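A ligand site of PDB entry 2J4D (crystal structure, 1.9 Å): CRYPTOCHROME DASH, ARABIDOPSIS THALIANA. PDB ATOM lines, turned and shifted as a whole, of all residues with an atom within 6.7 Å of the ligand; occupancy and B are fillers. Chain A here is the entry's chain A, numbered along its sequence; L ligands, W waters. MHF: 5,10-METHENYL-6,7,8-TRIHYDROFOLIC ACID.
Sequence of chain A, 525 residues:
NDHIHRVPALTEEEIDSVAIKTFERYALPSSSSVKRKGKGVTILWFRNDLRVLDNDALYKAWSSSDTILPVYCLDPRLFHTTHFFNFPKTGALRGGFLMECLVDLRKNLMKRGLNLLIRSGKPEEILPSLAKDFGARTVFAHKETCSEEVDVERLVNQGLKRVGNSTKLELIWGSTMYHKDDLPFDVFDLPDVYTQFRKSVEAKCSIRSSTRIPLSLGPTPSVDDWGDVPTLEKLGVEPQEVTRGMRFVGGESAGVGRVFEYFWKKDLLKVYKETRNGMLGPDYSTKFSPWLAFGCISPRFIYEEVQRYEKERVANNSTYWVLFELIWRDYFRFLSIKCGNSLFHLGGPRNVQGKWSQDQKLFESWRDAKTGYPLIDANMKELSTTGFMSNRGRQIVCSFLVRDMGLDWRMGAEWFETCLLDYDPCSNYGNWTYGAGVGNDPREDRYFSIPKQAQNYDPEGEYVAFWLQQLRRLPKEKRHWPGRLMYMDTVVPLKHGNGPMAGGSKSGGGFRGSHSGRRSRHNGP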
ATOM      1  N   THR A  82      25.640  14.576  23.412  1.00  0.00           N
ATOM      2  CA  THR A  82      24.872  14.106  22.264  1.00  0.00           C
ATOM      3  C   THR A  82      25.227  14.914  21.021  1.00  0.00           C
ATOM      4  O   THR A  82      25.691  16.056  21.114  1.00  0.00           O
ATOM      5  CB  THR A  82      23.352  14.140  22.538  1.00  0.00           C
ATOM      6  OG1 THR A  82      22.947  15.467  22.889  1.00  0.00           O
ATOM      7  CG2 THR A  82      23.015  13.188  23.683  1.00  0.00           C
ATOM      8  N   HIS A  83      25.015  14.300  19.876  1.00  0.00           N
ATOM      9  CA  HIS A  83      25.379  14.850  18.566  1.00  0.00           C
ATOM     10  C   HIS A  83      24.913  16.224  18.143  1.00  0.00           C
ATOM     11  O   HIS A  83      25.736  17.114  17.862  1.00  0.00           O
ATOM     12  CB  HIS A  83      24.988  13.825  17.491  1.00  0.00           C
ATOM     13  CG  HIS A  83      25.541  14.110  16.134  1.00  0.00           C
ATOM     14  ND1 HIS A  83      24.969  15.016  15.273  1.00  0.00           N
ATOM     15  CD2 HIS A  83      26.628  13.608  15.489  1.00  0.00           C
ATOM     16  CE1 HIS A  83      25.665  15.052  14.143  1.00  0.00           C
ATOM     17  NE2 HIS A  83      26.672  14.207  14.246  1.00  0.00           N
ATOM     18  N   PHE A  84      23.609  16.427  18.073  1.00  0.00           N
ATOM     19  CA  PHE A  84      23.062  17.698  17.636  1.00  0.00           C
ATOM     20  C   PHE A  84      22.822  18.745  18.717  1.00  0.00           C
ATOM     21  O   PHE A  84      23.101  19.915  18.494  1.00  0.00           O
ATOM     22  CB  PHE A  84      21.759  17.466  16.864  1.00  0.00           C
ATOM     23  CG  PHE A  84      21.951  16.756  15.550  1.00  0.00           C
ATOM     24  CD1 PHE A  84      22.564  17.402  14.484  1.00  0.00           C
ATOM     25  CD2 PHE A  84      21.536  15.434  15.390  1.00  0.00           C
ATOM     26  CE1 PHE A  84      22.765  16.733  13.263  1.00  0.00           C
ATOM     27  CE2 PHE A  84      21.735  14.760  14.178  1.00  0.00           C
ATOM     28  CZ  PHE A  84      22.351  15.413  13.117  1.00  0.00           C
ATOM     29  N   LYS A  89      26.059  12.574  26.881  1.00  0.00           N
ATOM     30  CA  LYS A  89      26.003  11.389  26.024  1.00  0.00           C
ATOM     31  C   LYS A  89      25.398  10.215  26.808  1.00  0.00           C
ATOM     32  O   LYS A  89      24.576   9.458  26.290  1.00  0.00           O
ATOM     33  CB  LYS A  89      27.397  11.040  25.502  1.00  0.00           C
ATOM     34  CG  LYS A  89      27.450   9.846  24.551  1.00  0.00           C
ATOM     35  CD  LYS A  89      26.655  10.076  23.256  1.00  0.00           C
ATOM     36  CE  LYS A  89      26.935   8.958  22.245  1.00  0.00           C
ATOM     37  NZ  LYS A  89      26.095   9.061  21.000  1.00  0.00           N
ATOM     38  N   CYS A 146      25.422   0.983  13.923  1.00  0.00           N
ATOM     39  CA  CYS A 146      25.422   2.419  13.641  1.00  0.00           C
ATOM     40  C   CYS A 146      26.775   3.080  13.485  1.00  0.00           C
ATOM     41  O   CYS A 146      27.800   2.587  13.962  1.00  0.00           O
ATOM     42  CB  CYS A 146      24.587   3.150  14.698  1.00  0.00           C
ATOM     43  SG  CYS A 146      22.872   2.566  14.721  1.00  0.00           S
ATOM     44  N   SER A 147      26.763   4.216  12.792  1.00  0.00           N
ATOM     45  CA  SER A 147      27.942   5.030  12.496  1.00  0.00           C
ATOM     46  C   SER A 147      29.057   5.093  13.543  1.00  0.00           C
ATOM     47  O   SER A 147      30.208   4.749  13.258  1.00  0.00           O
ATOM     48  CB  SER A 147      27.492   6.467  12.170  1.00  0.00           C
ATOM     49  OG  SER A 147      28.602   7.350  12.143  1.00  0.00           O
ATOM     50  N   GLU A 148      28.716   5.557  14.739  1.00  0.00           N
ATOM     51  CA  GLU A 148      29.702   5.699  15.803  1.00  0.00           C
ATOM     52  C   GLU A 148      30.394   4.396  16.174  1.00  0.00           C
ATOM     53  O   GLU A 148      31.626   4.344  16.273  1.00  0.00           O
ATOM     54  CB  GLU A 148      29.052   6.333  17.041  1.00  0.00           C
ATOM     55  CG  GLU A 148      28.739   7.805  16.855  1.00  0.00           C
ATOM     56  CD  GLU A 148      27.930   8.395  17.993  1.00  0.00           C
ATOM     57  OE1 GLU A 148      27.678   7.694  18.997  1.00  0.00           O
ATOM     58  OE2 GLU A 148      27.534   9.573  17.868  1.00  0.00           O
ATOM     59  N   GLU A 149      29.602   3.341  16.358  1.00  0.00           N
ATOM     60  CA  GLU A 149      30.149   2.047  16.742  1.00  0.00           C
ATOM     61  C   GLU A 149      30.979   1.397  15.618  1.00  0.00           C
ATOM     62  O   GLU A 149      32.001   0.779  15.882  1.00  0.00           O
ATOM     63  CB  GLU A 149      29.024   1.100  17.180  1.00  0.00           C
ATOM     64  CG  GLU A 149      28.404   1.481  18.520  1.00  0.00           C
ATOM     65  CD  GLU A 149      27.226   2.443  18.389  1.00  0.00           C
ATOM     66  OE1 GLU A 149      27.125   3.197  17.397  1.00  0.00           O
ATOM     67  OE2 GLU A 149      26.375   2.450  19.306  1.00  0.00           O
ATOM     68  N   VAL A 150      30.542   1.553  14.370  1.00  0.00           N
ATOM     69  CA  VAL A 150      31.295   0.951  13.276  1.00  0.00           C
ATOM     70  C   VAL A 150      32.580   1.734  13.017  1.00  0.00           C
ATOM     71  O   VAL A 150      33.566   1.200  12.514  1.00  0.00           O
ATOM     72  CB  VAL A 150      30.451   0.844  11.994  1.00  0.00           C
ATOM     73  CG1 VAL A 150      29.278  -0.124  12.245  1.00  0.00           C
ATOM     74  CG2 VAL A 150      29.937   2.205  11.577  1.00  0.00           C
ATOM     75  N   GLY A 340      21.227   3.544   7.548  1.00  0.00           N
ATOM     76  CA  GLY A 340      22.469   4.265   7.745  1.00  0.00           C
ATOM     77  C   GLY A 340      22.164   5.521   8.526  1.00  0.00           C
ATOM     78  O   GLY A 340      21.254   5.550   9.359  1.00  0.00           O
ATOM     79  N   ASN A 341      22.904   6.593   8.244  1.00  0.00           N
ATOM     80  CA  ASN A 341      22.710   7.837   8.965  1.00  0.00           C
ATOM     81  C   ASN A 341      21.420   8.602   8.685  1.00  0.00           C
ATOM     82  O   ASN A 341      21.157   9.613   9.314  1.00  0.00           O
ATOM     83  CB  ASN A 341      23.927   8.745   8.767  1.00  0.00           C
ATOM     84  CG  ASN A 341      25.200   8.110   9.283  1.00  0.00           C
ATOM     85  OD1 ASN A 341      25.186   7.417  10.306  1.00  0.00           O
ATOM     86  ND2 ASN A 341      26.308   8.344   8.590  1.00  0.00           N
ATOM     87  N   SER A 342      20.594   8.120   7.751  1.00  0.00           N
ATOM     88  CA  SER A 342      19.329   8.829   7.512  1.00  0.00           C
ATOM     89  C   SER A 342      18.446   8.619   8.754  1.00  0.00           C
ATOM     90  O   SER A 342      17.453   9.314   8.971  1.00  0.00           O
ATOM     91  CB  SER A 342      18.624   8.281   6.260  1.00  0.00           C
ATOM     92  OG  SER A 342      18.181   6.957   6.440  1.00  0.00           O
ATOM     93  N   PHE A 344      19.291   9.346  11.623  1.00  0.00           N
ATOM     94  CA  PHE A 344      19.518  10.469  12.522  1.00  0.00           C
ATOM     95  C   PHE A 344      19.234  11.840  11.924  1.00  0.00           C
ATOM     96  O   PHE A 344      19.284  12.850  12.632  1.00  0.00           O
ATOM     97  CB  PHE A 344      20.964  10.428  13.007  1.00  0.00           C
ATOM     98  CG  PHE A 344      21.395   9.068  13.482  1.00  0.00           C
ATOM     99  CD1 PHE A 344      20.853   8.518  14.644  1.00  0.00           C
ATOM    100  CD2 PHE A 344      22.378   8.345  12.797  1.00  0.00           C
ATOM    101  CE1 PHE A 344      21.272   7.269  15.120  1.00  0.00           C
ATOM    102  CE2 PHE A 344      22.816   7.093  13.250  1.00  0.00           C
ATOM    103  CZ  PHE A 344      22.268   6.554  14.418  1.00  0.00           C
ATOM    104  N   HIS A 345      18.945  11.881  10.628  1.00  0.00           N
ATOM    105  CA  HIS A 345      18.694  13.149   9.940  1.00  0.00           C
ATOM    106  C   HIS A 345      17.282  13.664  10.141  1.00  0.00           C
ATOM    107  O   HIS A 345      16.332  12.884  10.261  1.00  0.00           O
ATOM    108  CB  HIS A 345      18.997  12.970   8.453  1.00  0.00           C
ATOM    109  CG  HIS A 345      20.443  12.674   8.177  1.00  0.00           C
ATOM    110  ND1 HIS A 345      20.867  11.960   7.071  1.00  0.00           N
ATOM    111  CD2 HIS A 345      21.569  12.986   8.868  1.00  0.00           C
ATOM    112  CE1 HIS A 345      22.182  11.852   7.098  1.00  0.00           C
ATOM    113  NE2 HIS A 345      22.635  12.461   8.178  1.00  0.00           N
ATOM    114  N   GLU A 414      17.355  12.831  21.375  1.00  0.00           N
ATOM    115  CA  GLU A 414      18.621  12.969  22.097  1.00  0.00           C
ATOM    116  C   GLU A 414      18.406  13.005  23.603  1.00  0.00           C
ATOM    117  O   GLU A 414      19.266  12.551  24.369  1.00  0.00           O
ATOM    118  CB  GLU A 414      19.396  14.217  21.624  1.00  0.00           C
ATOM    119  CG  GLU A 414      20.113  13.983  20.284  1.00  0.00           C
ATOM    120  CD  GLU A 414      21.119  15.066  19.904  1.00  0.00           C
ATOM    121  OE1 GLU A 414      21.434  15.941  20.734  1.00  0.00           O
ATOM    122  OE2 GLU A 414      21.602  15.015  18.755  1.00  0.00           O
ATOM    123  N   GLU A 417      18.040   9.636  24.545  1.00  0.00           N
ATOM    124  CA  GLU A 417      19.376   9.039  24.505  1.00  0.00           C
ATOM    125  C   GLU A 417      20.131   9.310  25.810  1.00  0.00           C
ATOM    126  O   GLU A 417      20.843   8.451  26.336  1.00  0.00           O
ATOM    127  CB  GLU A 417      20.180   9.582  23.320  1.00  0.00           C
ATOM    128  CG  GLU A 417      21.657   9.129  23.363  1.00  0.00           C
ATOM    129  CD  GLU A 417      22.396   9.332  22.049  1.00  0.00           C
ATOM    130  OE1 GLU A 417      21.858   9.989  21.132  1.00  0.00           O
ATOM    131  OE2 GLU A 417      23.540   8.831  21.950  1.00  0.00           O
ATOM    132  N   TYR A 423      18.535   2.730  26.409  1.00  0.00           N
ATOM    133  CA  TYR A 423      18.868   3.418  25.177  1.00  0.00           C
ATOM    134  C   TYR A 423      19.609   2.502  24.218  1.00  0.00           C
ATOM    135  O   TYR A 423      20.602   1.879  24.572  1.00  0.00           O
ATOM    136  CB  TYR A 423      19.740   4.637  25.422  1.00  0.00           C
ATOM    137  CG  TYR A 423      20.301   5.171  24.117  1.00  0.00           C
ATOM    138  CD1 TYR A 423      19.452   5.710  23.152  1.00  0.00           C
ATOM    139  CD2 TYR A 423      21.668   5.099  23.834  1.00  0.00           C
ATOM    140  CE1 TYR A 423      19.943   6.160  21.922  1.00  0.00           C
ATOM    141  CE2 TYR A 423      22.169   5.546  22.604  1.00  0.00           C
ATOM    142  CZ  TYR A 423      21.296   6.075  21.663  1.00  0.00           C
ATOM    143  OH  TYR A 423      21.779   6.530  20.448  1.00  0.00           O
ATOM    144  N   ASP A 424      19.092   2.467  22.982  1.00  0.00           N
ATOM    145  CA  ASP A 424      19.637   1.675  21.896  1.00  0.00           C
ATOM    146  C   ASP A 424      19.454   2.582  20.683  1.00  0.00           C
ATOM    147  O   ASP A 424      18.336   3.026  20.401  1.00  0.00           O
ATOM    148  CB  ASP A 424      18.808   0.384  21.756  1.00  0.00           C
ATOM    149  CG  ASP A 424      19.287  -0.498  20.631  1.00  0.00           C
ATOM    150  OD1 ASP A 424      19.754  -1.620  20.921  1.00  0.00           O
ATOM    151  OD2 ASP A 424      19.196  -0.073  19.459  1.00  0.00           O
ATOM    152  N   PRO A 425      20.537   2.895  19.953  1.00  0.00           N
ATOM    153  CA  PRO A 425      20.326   3.777  18.804  1.00  0.00           C
ATOM    154  C   PRO A 425      19.299   3.308  17.788  1.00  0.00           C
ATOM    155  O   PRO A 425      18.490   4.102  17.308  1.00  0.00           O
ATOM    156  CB  PRO A 425      21.725   3.921  18.196  1.00  0.00           C
ATOM    157  CG  PRO A 425      22.408   2.643  18.608  1.00  0.00           C
ATOM    158  CD  PRO A 425      21.940   2.468  20.035  1.00  0.00           C
ATOM    159  N   CYS A 426      19.325   2.017  17.482  1.00  0.00           N
ATOM    160  CA  CYS A 426      18.411   1.445  16.504  1.00  0.00           C
ATOM    161  C   CYS A 426      16.961   1.594  16.936  1.00  0.00           C
ATOM    162  O   CYS A 426      16.124   2.080  16.184  1.00  0.00           O
ATOM    163  CB  CYS A 426      18.733  -0.042  16.297  1.00  0.00           C
ATOM    164  SG  CYS A 426      20.478  -0.382  15.942  1.00  0.00           S
ATOM    165  N   TYR A 429      16.072   5.839  17.894  1.00  0.00           N
ATOM    166  CA  TYR A 429      15.876   6.648  16.710  1.00  0.00           C
ATOM    167  C   TYR A 429      14.883   6.003  15.764  1.00  0.00           C
ATOM    168  O   TYR A 429      14.154   6.694  15.054  1.00  0.00           O
ATOM    169  CB  TYR A 429      17.226   6.925  16.060  1.00  0.00           C
ATOM    170  CG  TYR A 429      18.036   7.903  16.880  1.00  0.00           C
ATOM    171  CD1 TYR A 429      17.882   9.287  16.691  1.00  0.00           C
ATOM    172  CD2 TYR A 429      18.902   7.464  17.895  1.00  0.00           C
ATOM    173  CE1 TYR A 429      18.552  10.205  17.489  1.00  0.00           C
ATOM    174  CE2 TYR A 429      19.583   8.380  18.706  1.00  0.00           C
ATOM    175  CZ  TYR A 429      19.402   9.749  18.501  1.00  0.00           C
ATOM    176  OH  TYR A 429      20.052  10.672  19.285  1.00  0.00           O
HETATM  177  N1  MHF L   1      24.171   6.602  19.290  1.00  0.00           N
HETATM  178  C2  MHF L   1      24.872   5.469  18.965  1.00  0.00           C
HETATM  179  NA2 MHF L   1      24.923   4.445  19.868  1.00  0.00           N
HETATM  180  N3  MHF L   1      25.493   5.334  17.786  1.00  0.00           N
HETATM  181  C4  MHF L   1      25.489   6.345  16.858  1.00  0.00           C
HETATM  182  O4  MHF L   1      26.076   6.217  15.788  1.00  0.00           O
HETATM  183  C4A MHF L   1      24.795   7.556  17.165  1.00  0.00           C
HETATM  184  N5  MHF L   1      24.752   8.684  16.312  1.00  0.00           N
HETATM  185  C6  MHF L   1      24.321  10.042  16.790  1.00  0.00           C
HETATM  186  C7  MHF L   1      23.041   9.816  17.627  1.00  0.00           C
HETATM  187  N8  MHF L   1      23.419   8.848  18.700  1.00  0.00           N
HETATM  188  C8A MHF L   1      24.115   7.668  18.403  1.00  0.00           C
HETATM  189  C9  MHF L   1      24.159  10.925  15.529  1.00  0.00           C
HETATM  190  N10 MHF L   1      24.360   9.950  14.428  1.00  0.00           N
HETATM  191  C11 MHF L   1      25.252   8.912  14.953  1.00  0.00           C
HETATM  192  C12 MHF L   1      25.819  11.583  10.724  1.00  0.00           C
HETATM  193  C13 MHF L   1      24.687  12.134  11.381  1.00  0.00           C
HETATM  194  C14 MHF L   1      24.233  11.615  12.595  1.00  0.00           C
HETATM  195  C15 MHF L   1      24.905  10.518  13.206  1.00  0.00           C
HETATM  196  C16 MHF L   1      26.083   9.974  12.551  1.00  0.00           C
HETATM  197  C17 MHF L   1      26.529  10.502  11.329  1.00  0.00           C
HETATM  198  C   MHF L   1      26.237  12.135   9.402  1.00  0.00           C
HETATM  199  O   MHF L   1      25.579  13.050   8.913  1.00  0.00           O
HETATM  200  N   MHF L   1      27.294  11.640   8.730  1.00  0.00           N
HETATM  201  CA  MHF L   1      27.656  12.184   7.428  1.00  0.00           C
HETATM  202  CB  MHF L   1      29.153  12.025   7.173  1.00  0.00           C
HETATM  203  CG  MHF L   1      30.029  12.722   8.181  1.00  0.00           C
HETATM  204  CD  MHF L   1      29.753  14.207   8.248  1.00  0.00           C
HETATM  205  OE1 MHF L   1      30.085  14.916   7.278  1.00  0.00           O
HETATM  206  OE2 MHF L   1      29.186  14.655   9.274  1.00  0.00           O
HETATM  207  CT  MHF L   1      26.876  11.469   6.328  1.00  0.00           C
HETATM  208  O1  MHF L   1      26.293  10.392   6.603  1.00  0.00           O
HETATM  209  O2  MHF L   1      26.850  11.980   5.182  1.00  0.00           O
HETATM  210  O   HOH W   1      27.996  10.843  15.745  1.00  0.00           O
HETATM  211  O   HOH W   2      23.820  10.199   5.091  1.00  0.00           O
HETATM  212  O   HOH W   3      24.269  14.019   5.177  1.00  0.00           O
HETATM  213  O   HOH W   4      25.802   5.318  23.009  1.00  0.00           O
HETATM  214  O   HOH W   5      24.946   2.969  22.581  1.00  0.00           O
HETATM  215  O   HOH W   6      31.675  14.058   5.100  1.00  0.00           O
HETATM  216  O   HOH W   7      23.796  11.881  20.215  1.00  0.00           O
HETATM  217  O   HOH W   8      23.529  15.466  10.042  1.00  0.00           O
HETATM  218  O   HOH W   9      24.479  15.471   7.481  1.00  0.00           O
HETATM  219  O   HOH W  10      21.101  12.534  17.366  1.00  0.00           O
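The side-chain carboxylate of Glu 149 is in hydrogen-bond range of a nitrogen (NA2) of the ligand (2.5 Å).
N1 of the ligand is in hydrogen-bond range of OH of Tyr 423.
O1 of the ligand is in hydrogen-bond range of ND2 of Asn 341 (2.9 Å).
N of Glu 148 sits at hydrogen-bond distance from O4 of the ligand (2.9 Å).
OE1 of Glu 148 lies close to N3 of the ligand (3.4 Å).
A ring nitrogen (NE2) of His 345 lies within hydrogen-bond range of an oxygen (O) of the ligand, 3.1 Å away.
A nitrogen (N8) of the ligand is in hydrogen-bond range of the side-chain carboxylate (OE1) of Glu 417 (3.1 Å).
The side-chain hydroxyl of Tyr 423 lies within hydrogen-bond range of the side-chain carboxylate of Glu 417.
The backbone carbonyl oxygen of Asn 341 is in hydrogen-bond range of a ring nitrogen (ND1) of His 345, 3.3 Å away.
The side-chain carboxylate (OE1) of Glu 148 lies within salt-bridge range of the side-chain amino group (NZ) of Lys 89 (2.9 Å).
OE1 of Glu 417 lies within hydrogen-bond range of OH of Tyr 429.
OE2 of Glu 417 is in salt-bridge range of NZ of Lys 89, at 2.7 Å.
Water W10 lies within hydrogen-bond range of OH of Tyr 429 and OE2 of Glu 414.
Water W7 lies within hydrogen-bond range of N of His 83 (2.7 Å), OE1 of Glu 417 (2.9 Å) and N8 of the ligand (3.4 Å).
Merely in contact with the ligand: Phe 344 (3.0 Å), Pro 425 (3.3 Å), Tyr 429 (3.5 Å), His 83 (3.5 Å), Lys 89 (3.5 Å), Cys 146 (3.6 Å) and Ser 147 (3.7 Å).
Hydrophobic or aromatic side chains within 4 Å of the ligand: His 83, Phe 344, Tyr 423, Pro 425 and Tyr 429.
Of the 21 residues printed, 13 come within 4 Å of the ligand.
The nearest printed residue that does not touch the ligand is Phe 84 (4.3 Å).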
